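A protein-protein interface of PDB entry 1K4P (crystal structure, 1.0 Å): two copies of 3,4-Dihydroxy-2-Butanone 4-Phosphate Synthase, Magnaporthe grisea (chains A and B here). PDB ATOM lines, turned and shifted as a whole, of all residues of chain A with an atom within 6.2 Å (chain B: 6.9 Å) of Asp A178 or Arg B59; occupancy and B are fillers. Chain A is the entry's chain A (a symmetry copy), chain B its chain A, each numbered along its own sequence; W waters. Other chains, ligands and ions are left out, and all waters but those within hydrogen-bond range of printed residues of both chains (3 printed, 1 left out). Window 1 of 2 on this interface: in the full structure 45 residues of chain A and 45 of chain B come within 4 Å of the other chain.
The side-chain carboxylate of Asp B178 is in salt-bridge range of the guanidinium group of Arg B59, 3.6 Å away.
O of Asp B178 sits at hydrogen-bond distance from NE of Arg B188 (2.8 Å).
The guanidinium group (NH1) of Arg A59 is in salt-bridge range of the side-chain carboxylate (OD1) of Asp A178.
O of Asp A178 lies within hydrogen-bond range of NE of Arg A188, 2.8 Å away.
The guanidinium group (NH2) of Arg A188 lies within hydrogen-bond range of the backbone carbonyl oxygen (O) of Gly A179 (3.0 Å).
Among the printed residues, merely in contact across the chains: Val A58 with Ser B62 (3.6 Å), Arg A59 with Arg B59 (3.4 Å), Arg A59 with Asp B178 (3.5 Å), Asp A178 with Arg B59 (3.5 Å), Arg A188 with Ala B55 (3.7 Å), Arg A188 with Phe B56 (3.5 Å) and Pro A191 with Ala B55 (3.4 Å).
Asp A178 touches one residue of chain B.
Of the printed residues of chain B, Pro A191 touches Ala B55.
Of the printed residues of chain A, Phe B56 touches Arg A188.
Val B58 touches none of the printed residues of chain A.
Of the printed residues of chain A, Arg B59 touches Arg A59 and Asp A178.
Ser B61 touches none of the printed residues of chain A.
The nearest printed residue of chain A that does not touch Arg B59 is Arg A188 (4.02 Å).
Printed residues of chain A that touch a printed residue of chain B: Val A58, Arg A59, Asp A178, Arg A188 and Pro A191.
Of the 14 printed residues of chain B, 5 touch a printed residue of chain A.
Printed residues of chain B that touch a printed residue of chain A: Ala B55, Phe B56, Arg B59, Ser B62 and Asp B178.
Hydrophobic or aromatic side chains of chain B that line the printed part of chain A: Ala B55 and Phe B56.
Among the printed residues, 7 pairs touch across the chains.
Among the printed residues, no Asp or Glu carboxylate lies within 4 Å of a Lys or Arg side-chain nitrogen of the other chain.
Arg B59 touches its own counterpart, Arg A59.
Arg A59 touches Asp B178, and with the chains exchanged Asp A178 touches Arg B59.
Of the 7 pairs that touch across the chains among the printed residues, 3 have their exchanged pair printed and touching as well.
Water W2 lies within hydrogen-bond range of O of Ala B55 (2.8 Å) and OD2 of Asp A178 (2.9 Å).
Water W3 bridges the guanidinium group of Arg A188 (2.9 Å) and a ring nitrogen (NE2) of His B60 (2.9 Å).
Water W1 lies within hydrogen-bond range of NH1 of Arg B188 (2.9 Å) and NE2 of His A60 (2.9 Å).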
ATOM      1  N   VAL A  58      -6.162   8.923  23.045  1.00  0.00           N
ATOM      2  CA  VAL A  58      -6.556   7.762  22.276  1.00  0.00           C
ATOM      3  C   VAL A  58      -5.961   7.811  20.896  1.00  0.00           C
ATOM      4  O   VAL A  58      -5.486   6.801  20.359  1.00  0.00           O
ATOM      5  CB  VAL A  58      -8.079   7.657  22.252  1.00  0.00           C
ATOM      6  CG1 VAL A  58      -8.543   6.520  21.323  1.00  0.00           C
ATOM      7  CG2 VAL A  58      -8.636   7.364  23.652  1.00  0.00           C
ATOM      8  N   ARG A  59      -5.982   9.012  20.291  1.00  0.00           N
ATOM      9  CA  ARG A  59      -5.456   9.146  18.933  1.00  0.00           C
ATOM     10  C   ARG A  59      -3.992   8.777  18.774  1.00  0.00           C
ATOM     11  O   ARG A  59      -3.610   8.187  17.731  1.00  0.00           O
ATOM     12  CB  ARG A  59      -5.709  10.565  18.463  1.00  0.00           C
ATOM     13  CG  ARG A  59      -4.934  10.969  17.191  1.00  0.00           C
ATOM     14  CD  ARG A  59      -5.483  10.286  15.940  1.00  0.00           C
ATOM     15  NE  ARG A  59      -4.703  10.745  14.797  1.00  0.00           N
ATOM     16  CZ  ARG A  59      -3.444  10.362  14.572  1.00  0.00           C
ATOM     17  NH1 ARG A  59      -2.775   9.463  15.309  1.00  0.00           N
ATOM     18  NH2 ARG A  59      -2.839  10.887  13.525  1.00  0.00           N
ATOM     19  N   HIS A  60      -3.170   9.173  19.733  1.00  0.00           N
ATOM     20  CA  HIS A  60      -1.743   8.974  19.619  1.00  0.00           C
ATOM     21  C   HIS A  60      -1.176   7.789  20.402  1.00  0.00           C
ATOM     22  O   HIS A  60       0.025   7.525  20.365  1.00  0.00           O
ATOM     23  CB  HIS A  60      -1.005  10.256  20.002  1.00  0.00           C
ATOM     24  CG  HIS A  60      -1.318  11.363  19.059  1.00  0.00           C
ATOM     25  ND1 HIS A  60      -0.753  11.426  17.790  1.00  0.00           N
ATOM     26  CD2 HIS A  60      -2.152  12.438  19.201  1.00  0.00           C
ATOM     27  CE1 HIS A  60      -1.254  12.496  17.193  1.00  0.00           C
ATOM     28  NE2 HIS A  60      -2.103  13.121  17.996  1.00  0.00           N
ATOM     29  N   SER A  61      -2.036   7.076  21.114  1.00  0.00           N
ATOM     30  CA  SER A  61      -1.538   5.953  21.897  1.00  0.00           C
ATOM     31  C   SER A  61      -2.092   4.643  21.381  1.00  0.00           C
ATOM     32  O   SER A  61      -2.830   4.582  20.407  1.00  0.00           O
ATOM     33  CB  SER A  61      -1.953   6.073  23.383  1.00  0.00           C
ATOM     34  OG  SER A  61      -3.362   5.861  23.584  1.00  0.00           O
ATOM     35  N   VAL A 176       2.377   5.040  20.396  1.00  0.00           N
ATOM     36  CA  VAL A 176       2.734   4.171  19.293  1.00  0.00           C
ATOM     37  C   VAL A 176       3.244   4.968  18.107  1.00  0.00           C
ATOM     38  O   VAL A 176       3.116   6.190  18.076  1.00  0.00           O
ATOM     39  CB  VAL A 176       1.495   3.368  18.854  1.00  0.00           C
ATOM     40  CG1 VAL A 176       0.976   2.533  20.012  1.00  0.00           C
ATOM     41  CG2 VAL A 176       0.386   4.261  18.287  1.00  0.00           C
ATOM     42  N   ASP A 177       3.834   4.223  17.146  1.00  0.00           N
ATOM     43  CA  ASP A 177       4.190   4.781  15.873  1.00  0.00           C
ATOM     44  C   ASP A 177       3.022   4.247  14.978  1.00  0.00           C
ATOM     45  O   ASP A 177       2.982   3.046  14.677  1.00  0.00           O
ATOM     46  CB  ASP A 177       5.576   4.345  15.389  1.00  0.00           C
ATOM     47  CG  ASP A 177       5.877   4.938  14.016  1.00  0.00           C
ATOM     48  OD1 ASP A 177       5.030   5.434  13.270  1.00  0.00           O
ATOM     49  OD2 ASP A 177       7.150   4.903  13.719  1.00  0.00           O
ATOM     50  N   ASP A 178       2.021   5.073  14.612  1.00  0.00           N
ATOM     51  CA  ASP A 178       0.915   4.529  13.785  1.00  0.00           C
ATOM     52  C   ASP A 178       1.322   4.310  12.324  1.00  0.00           C
ATOM     53  O   ASP A 178       0.514   3.862  11.533  1.00  0.00           O
ATOM     54  CB  ASP A 178      -0.589   4.968  13.980  1.00  0.00           C
ATOM     55  CG  ASP A 178      -1.176   5.476  15.321  1.00  0.00           C
ATOM     56  OD1 ASP A 178      -0.779   6.543  15.812  1.00  0.00           O
ATOM     57  OD2 ASP A 178      -2.245   4.778  15.841  1.00  0.00           O
ATOM     58  N   GLY A 179       2.594   4.570  11.954  1.00  0.00           N
ATOM     59  CA  GLY A 179       3.031   4.342  10.580  1.00  0.00           C
ATOM     60  C   GLY A 179       2.425   5.375   9.638  1.00  0.00           C
ATOM     61  O   GLY A 179       2.013   6.438  10.037  1.00  0.00           O
ATOM     62  N   GLN A 180       2.347   5.045   8.366  1.00  0.00           N
ATOM     63  CA  GLN A 180       1.825   6.015   7.442  1.00  0.00           C
ATOM     64  C   GLN A 180       0.553   5.533   6.768  1.00  0.00           C
ATOM     65  O   GLN A 180       0.411   4.333   6.538  1.00  0.00           O
ATOM     66  CB  GLN A 180       2.873   6.236   6.309  1.00  0.00           C
ATOM     67  CG  GLN A 180       4.265   6.810   6.730  1.00  0.00           C
ATOM     68  CD  GLN A 180       5.338   5.734   6.970  1.00  0.00           C
ATOM     69  OE1 GLN A 180       5.825   5.556   8.100  1.00  0.00           O
ATOM     70  NE2 GLN A 180       5.752   5.031   5.914  1.00  0.00           N
ATOM     71  N   GLU A 181      -0.311   6.495   6.456  1.00  0.00           N
ATOM     72  CA  GLU A 181      -1.530   6.149   5.718  1.00  0.00           C
ATOM     73  C   GLU A 181      -1.139   5.538   4.376  1.00  0.00           C
ATOM     74  O   GLU A 181      -0.113   5.944   3.807  1.00  0.00           O
ATOM     75  CB  GLU A 181      -2.394   7.418   5.400  1.00  0.00           C
ATOM     76  CG  GLU A 181      -3.579   7.154   4.436  1.00  0.00           C
ATOM     77  CD  GLU A 181      -4.423   8.364   4.056  1.00  0.00           C
ATOM     78  OE1 GLU A 181      -4.114   9.503   4.333  1.00  0.00           O
ATOM     79  OE2 GLU A 181      -5.536   8.120   3.407  1.00  0.00           O
ATOM     80  N   ARG A 188      -1.661   0.280   7.545  1.00  0.00           N
ATOM     81  CA  ARG A 188      -0.774   1.405   7.765  1.00  0.00           C
ATOM     82  C   ARG A 188       0.610   0.852   7.506  1.00  0.00           C
ATOM     83  O   ARG A 188       0.930  -0.230   7.973  1.00  0.00           O
ATOM     84  CB  ARG A 188      -0.760   2.058   9.139  1.00  0.00           C
ATOM     85  CG  ARG A 188      -2.139   2.400   9.645  1.00  0.00           C
ATOM     86  CD  ARG A 188      -2.548   3.833   9.446  1.00  0.00           C
ATOM     87  NE  ARG A 188      -1.582   4.815   9.950  1.00  0.00           N
ATOM     88  CZ  ARG A 188      -1.796   6.124   9.692  1.00  0.00           C
ATOM     89  NH1 ARG A 188      -2.895   6.525   9.026  1.00  0.00           N
ATOM     90  NH2 ARG A 188      -0.909   7.039  10.108  1.00  0.00           N
ATOM     91  N   ALA A 189       1.433   1.607   6.831  1.00  0.00           N
ATOM     92  CA  ALA A 189       2.778   1.162   6.543  1.00  0.00           C
ATOM     93  C   ALA A 189       3.810   1.472   7.652  1.00  0.00           C
ATOM     94  O   ALA A 189       3.827   2.547   8.236  1.00  0.00           O
ATOM     95  CB  ALA A 189       3.184   1.911   5.263  1.00  0.00           C
ATOM     96  N   ALA A 190       4.671   0.509   7.900  1.00  0.00           N
ATOM     97  CA  ALA A 190       5.772   0.678   8.854  1.00  0.00           C
ATOM     98  C   ALA A 190       5.349   1.118  10.238  1.00  0.00           C
ATOM     99  O   ALA A 190       5.926   2.056  10.768  1.00  0.00           O
ATOM    100  CB  ALA A 190       6.763   1.725   8.321  1.00  0.00           C
ATOM    101  N   PRO A 191       4.376   0.464  10.850  1.00  0.00           N
ATOM    102  CA  PRO A 191       3.978   0.860  12.210  1.00  0.00           C
ATOM    103  C   PRO A 191       4.972   0.322  13.256  1.00  0.00           C
ATOM    104  O   PRO A 191       5.825  -0.482  12.951  1.00  0.00           O
ATOM    105  CB  PRO A 191       2.646   0.176  12.464  1.00  0.00           C
ATOM    106  CG  PRO A 191       2.773  -1.082  11.607  1.00  0.00           C
ATOM    107  CD  PRO A 191       3.650  -0.749  10.394  1.00  0.00           C
ATOM    108  N   GLY A 192       4.842   0.771  14.503  1.00  0.00           N
ATOM    109  CA  GLY A 192       5.733   0.289  15.566  1.00  0.00           C
ATOM    110  C   GLY A 192       5.407   1.018  16.882  1.00  0.00           C
ATOM    111  O   GLY A 192       4.273   1.430  17.131  1.00  0.00           O
ATOM    112  N   GLN B  53      -2.523  -4.361   9.083  1.00  0.00           N
ATOM    113  CA  GLN B  53      -3.962  -4.241   9.277  1.00  0.00           C
ATOM    114  C   GLN B  53      -4.252  -3.821  10.728  1.00  0.00           C
ATOM    115  O   GLN B  53      -5.115  -2.985  10.985  1.00  0.00           O
ATOM    116  CB  GLN B  53      -4.682  -5.581   9.031  1.00  0.00           C
ATOM    117  CG  GLN B  53      -4.750  -5.878   7.508  1.00  0.00           C
ATOM    118  CD  GLN B  53      -5.506  -7.160   7.235  1.00  0.00           C
ATOM    119  OE1 GLN B  53      -5.231  -8.196   7.866  1.00  0.00           O
ATOM    120  NE2 GLN B  53      -6.449  -7.108   6.309  1.00  0.00           N
ATOM    121  N   MET B  54      -3.569  -4.458  11.666  1.00  0.00           N
ATOM    122  CA  MET B  54      -3.797  -4.120  13.078  1.00  0.00           C
ATOM    123  C   MET B  54      -3.450  -2.650  13.354  1.00  0.00           C
ATOM    124  O   MET B  54      -4.139  -1.969  14.125  1.00  0.00           O
ATOM    125  CB  MET B  54      -2.969  -5.073  13.971  1.00  0.00           C
ATOM    126  CG  MET B  54      -3.196  -4.820  15.463  1.00  0.00           C
ATOM    127  SD  MET B  54      -4.918  -5.066  16.036  1.00  0.00           S
ATOM    128  CE  MET B  54      -5.027  -6.874  15.882  1.00  0.00           C
ATOM    129  N   ALA B  55      -2.399  -2.136  12.688  1.00  0.00           N
ATOM    130  CA  ALA B  55      -2.016  -0.742  12.875  1.00  0.00           C
ATOM    131  C   ALA B  55      -3.137   0.173  12.418  1.00  0.00           C
ATOM    132  O   ALA B  55      -3.422   1.210  13.039  1.00  0.00           O
ATOM    133  CB  ALA B  55      -0.713  -0.368  12.179  1.00  0.00           C
ATOM    134  N   PHE B  56      -3.776  -0.196  11.313  1.00  0.00           N
ATOM    135  CA  PHE B  56      -4.898   0.579  10.815  1.00  0.00           C
ATOM    136  C   PHE B  56      -6.038   0.512  11.822  1.00  0.00           C
ATOM    137  O   PHE B  56      -6.659   1.527  12.146  1.00  0.00           O
ATOM    138  CB  PHE B  56      -5.360   0.042   9.418  1.00  0.00           C
ATOM    139  CG  PHE B  56      -6.569   0.755   8.863  1.00  0.00           C
ATOM    140  CD1 PHE B  56      -6.397   1.878   8.049  1.00  0.00           C
ATOM    141  CD2 PHE B  56      -7.869   0.316   9.138  1.00  0.00           C
ATOM    142  CE1 PHE B  56      -7.494   2.569   7.534  1.00  0.00           C
ATOM    143  CE2 PHE B  56      -8.982   0.996   8.621  1.00  0.00           C
ATOM    144  CZ  PHE B  56      -8.792   2.116   7.807  1.00  0.00           C
ATOM    145  N   MET B  57      -6.306  -0.717  12.337  1.00  0.00           N
ATOM    146  CA  MET B  57      -7.389  -0.860  13.310  1.00  0.00           C
ATOM    147  C   MET B  57      -7.145   0.001  14.547  1.00  0.00           C
ATOM    148  O   MET B  57      -8.060   0.700  14.985  1.00  0.00           O
ATOM    149  CB  MET B  57      -7.508  -2.351  13.690  1.00  0.00           C
ATOM    150  CG  MET B  57      -8.857  -2.696  14.317  1.00  0.00           C
ATOM    151  SD  MET B  57      -8.878  -4.472  14.722  1.00  0.00           S
ATOM    152  CE  MET B  57     -10.673  -4.714  14.679  1.00  0.00           C
ATOM    153  N   VAL B  58      -5.922  -0.010  15.072  1.00  0.00           N
ATOM    154  CA  VAL B  58      -5.632   0.789  16.244  1.00  0.00           C
ATOM    155  C   VAL B  58      -5.789   2.253  15.941  1.00  0.00           C
ATOM    156  O   VAL B  58      -6.332   3.026  16.743  1.00  0.00           O
ATOM    157  CB  VAL B  58      -4.240   0.446  16.766  1.00  0.00           C
ATOM    158  CG1 VAL B  58      -3.835   1.377  17.924  1.00  0.00           C
ATOM    159  CG2 VAL B  58      -4.185  -0.994  17.294  1.00  0.00           C
ATOM    160  N   ARG B  59      -5.302   2.662  14.756  1.00  0.00           N
ATOM    161  CA  ARG B  59      -5.379   4.077  14.393  1.00  0.00           C
ATOM    162  C   ARG B  59      -6.785   4.646  14.331  1.00  0.00           C
ATOM    163  O   ARG B  59      -6.997   5.822  14.721  1.00  0.00           O
ATOM    164  CB  ARG B  59      -4.659   4.269  13.073  1.00  0.00           C
ATOM    165  CG  ARG B  59      -4.924   5.626  12.387  1.00  0.00           C
ATOM    166  CD  ARG B  59      -4.238   6.782  13.112  1.00  0.00           C
ATOM    167  NE  ARG B  59      -4.530   8.009  12.381  1.00  0.00           N
ATOM    168  CZ  ARG B  59      -5.730   8.592  12.384  1.00  0.00           C
ATOM    169  NH1 ARG B  59      -6.781   8.177  13.108  1.00  0.00           N
ATOM    170  NH2 ARG B  59      -5.870   9.674  11.644  1.00  0.00           N
ATOM    171  N   HIS B  60      -7.715   3.878  13.785  1.00  0.00           N
ATOM    172  CA  HIS B  60      -9.057   4.371  13.572  1.00  0.00           C
ATOM    173  C   HIS B  60     -10.096   3.925  14.602  1.00  0.00           C
ATOM    174  O   HIS B  60     -11.266   4.297  14.519  1.00  0.00           O
ATOM    175  CB  HIS B  60      -9.527   4.012  12.163  1.00  0.00           C
ATOM    176  CG  HIS B  60      -8.698   4.684  11.128  1.00  0.00           C
ATOM    177  ND1 HIS B  60      -8.855   6.034  10.828  1.00  0.00           N
ATOM    178  CD2 HIS B  60      -7.696   4.192  10.338  1.00  0.00           C
ATOM    179  CE1 HIS B  60      -7.957   6.333   9.902  1.00  0.00           C
ATOM    180  NE2 HIS B  60      -7.236   5.265   9.591  1.00  0.00           N
ATOM    181  N   SER B  61      -9.674   3.127  15.570  1.00  0.00           N
ATOM    182  CA  SER B  61     -10.634   2.656  16.560  1.00  0.00           C
ATOM    183  C   SER B  61     -10.304   3.192  17.935  1.00  0.00           C
ATOM    184  O   SER B  61      -9.364   3.949  18.135  1.00  0.00           O
ATOM    185  CB  SER B  61     -10.631   1.111  16.657  1.00  0.00           C
ATOM    186  OG  SER B  61      -9.433   0.595  17.265  1.00  0.00           O
ATOM    187  N   SER B  62     -11.093   2.707  18.918  1.00  0.00           N
ATOM    188  CA  SER B  62     -10.853   3.047  20.298  1.00  0.00           C
ATOM    189  C   SER B  62      -9.505   2.511  20.752  1.00  0.00           C
ATOM    190  O   SER B  62      -8.950   2.951  21.784  1.00  0.00           O
ATOM    191  CB  SER B  62     -11.955   2.452  21.187  1.00  0.00           C
ATOM    192  OG  SER B  62     -11.866   1.032  21.138  1.00  0.00           O
ATOM    193  N   GLY B  63      -8.952   1.506  20.050  1.00  0.00           N
ATOM    194  CA  GLY B  63      -7.678   0.915  20.489  1.00  0.00           C
ATOM    195  C   GLY B  63      -7.911  -0.216  21.516  1.00  0.00           C
ATOM    196  O   GLY B  63      -6.930  -0.906  21.881  1.00  0.00           O
ATOM    197  N   VAL B 176     -14.077   5.198  16.249  1.00  0.00           N
ATOM    198  CA  VAL B 176     -14.319   6.464  16.911  1.00  0.00           C
ATOM    199  C   VAL B 176     -14.263   7.618  15.928  1.00  0.00           C
ATOM    200  O   VAL B 176     -13.831   7.447  14.790  1.00  0.00           O
ATOM    201  CB  VAL B 176     -13.248   6.686  17.995  1.00  0.00           C
ATOM    202  CG1 VAL B 176     -13.297   5.561  19.016  1.00  0.00           C
ATOM    203  CG2 VAL B 176     -11.839   6.829  17.410  1.00  0.00           C
ATOM    204  N   ASP B 178     -12.133  10.648  15.938  1.00  0.00           N
ATOM    205  CA  ASP B 178     -11.013  11.239  16.713  1.00  0.00           C
ATOM    206  C   ASP B 178     -11.039  12.771  16.713  1.00  0.00           C
ATOM    207  O   ASP B 178     -10.182  13.389  17.316  1.00  0.00           O
ATOM    208  CB  ASP B 178      -9.562  10.616  16.722  1.00  0.00           C
ATOM    209  CG  ASP B 178      -9.262   9.114  16.486  1.00  0.00           C
ATOM    210  OD1 ASP B 178      -9.501   8.596  15.385  1.00  0.00           O
ATOM    211  OD2 ASP B 178      -8.590   8.445  17.486  1.00  0.00           O
ATOM    212  N   ARG B 188      -7.952  17.162  21.092  1.00  0.00           N
ATOM    213  CA  ARG B 188      -8.554  17.017  19.782  1.00  0.00           C
ATOM    214  C   ARG B 188      -9.905  17.688  19.910  1.00  0.00           C
ATOM    215  O   ARG B 188     -10.602  17.470  20.889  1.00  0.00           O
ATOM    216  CB  ARG B 188      -8.786  15.614  19.242  1.00  0.00           C
ATOM    217  CG  ARG B 188      -7.562  14.737  19.330  1.00  0.00           C
ATOM    218  CD  ARG B 188      -6.769  14.628  18.057  1.00  0.00           C
ATOM    219  NE  ARG B 188      -7.560  14.251  16.880  1.00  0.00           N
ATOM    220  CZ  ARG B 188      -6.963  14.265  15.669  1.00  0.00           C
ATOM    221  NH1 ARG B 188      -5.658  14.573  15.546  1.00  0.00           N
ATOM    222  NH2 ARG B 188      -7.672  13.962  14.573  1.00  0.00           N
HETATM  223  O   HOH W   1      -3.543  15.511  17.242  1.00  0.00           O
HETATM  224  O   HOH W   2      -1.557   2.148  14.960  1.00  0.00           O
HETATM  225  O   HOH W   3      -5.094   5.298   7.651  1.00  0.00           O
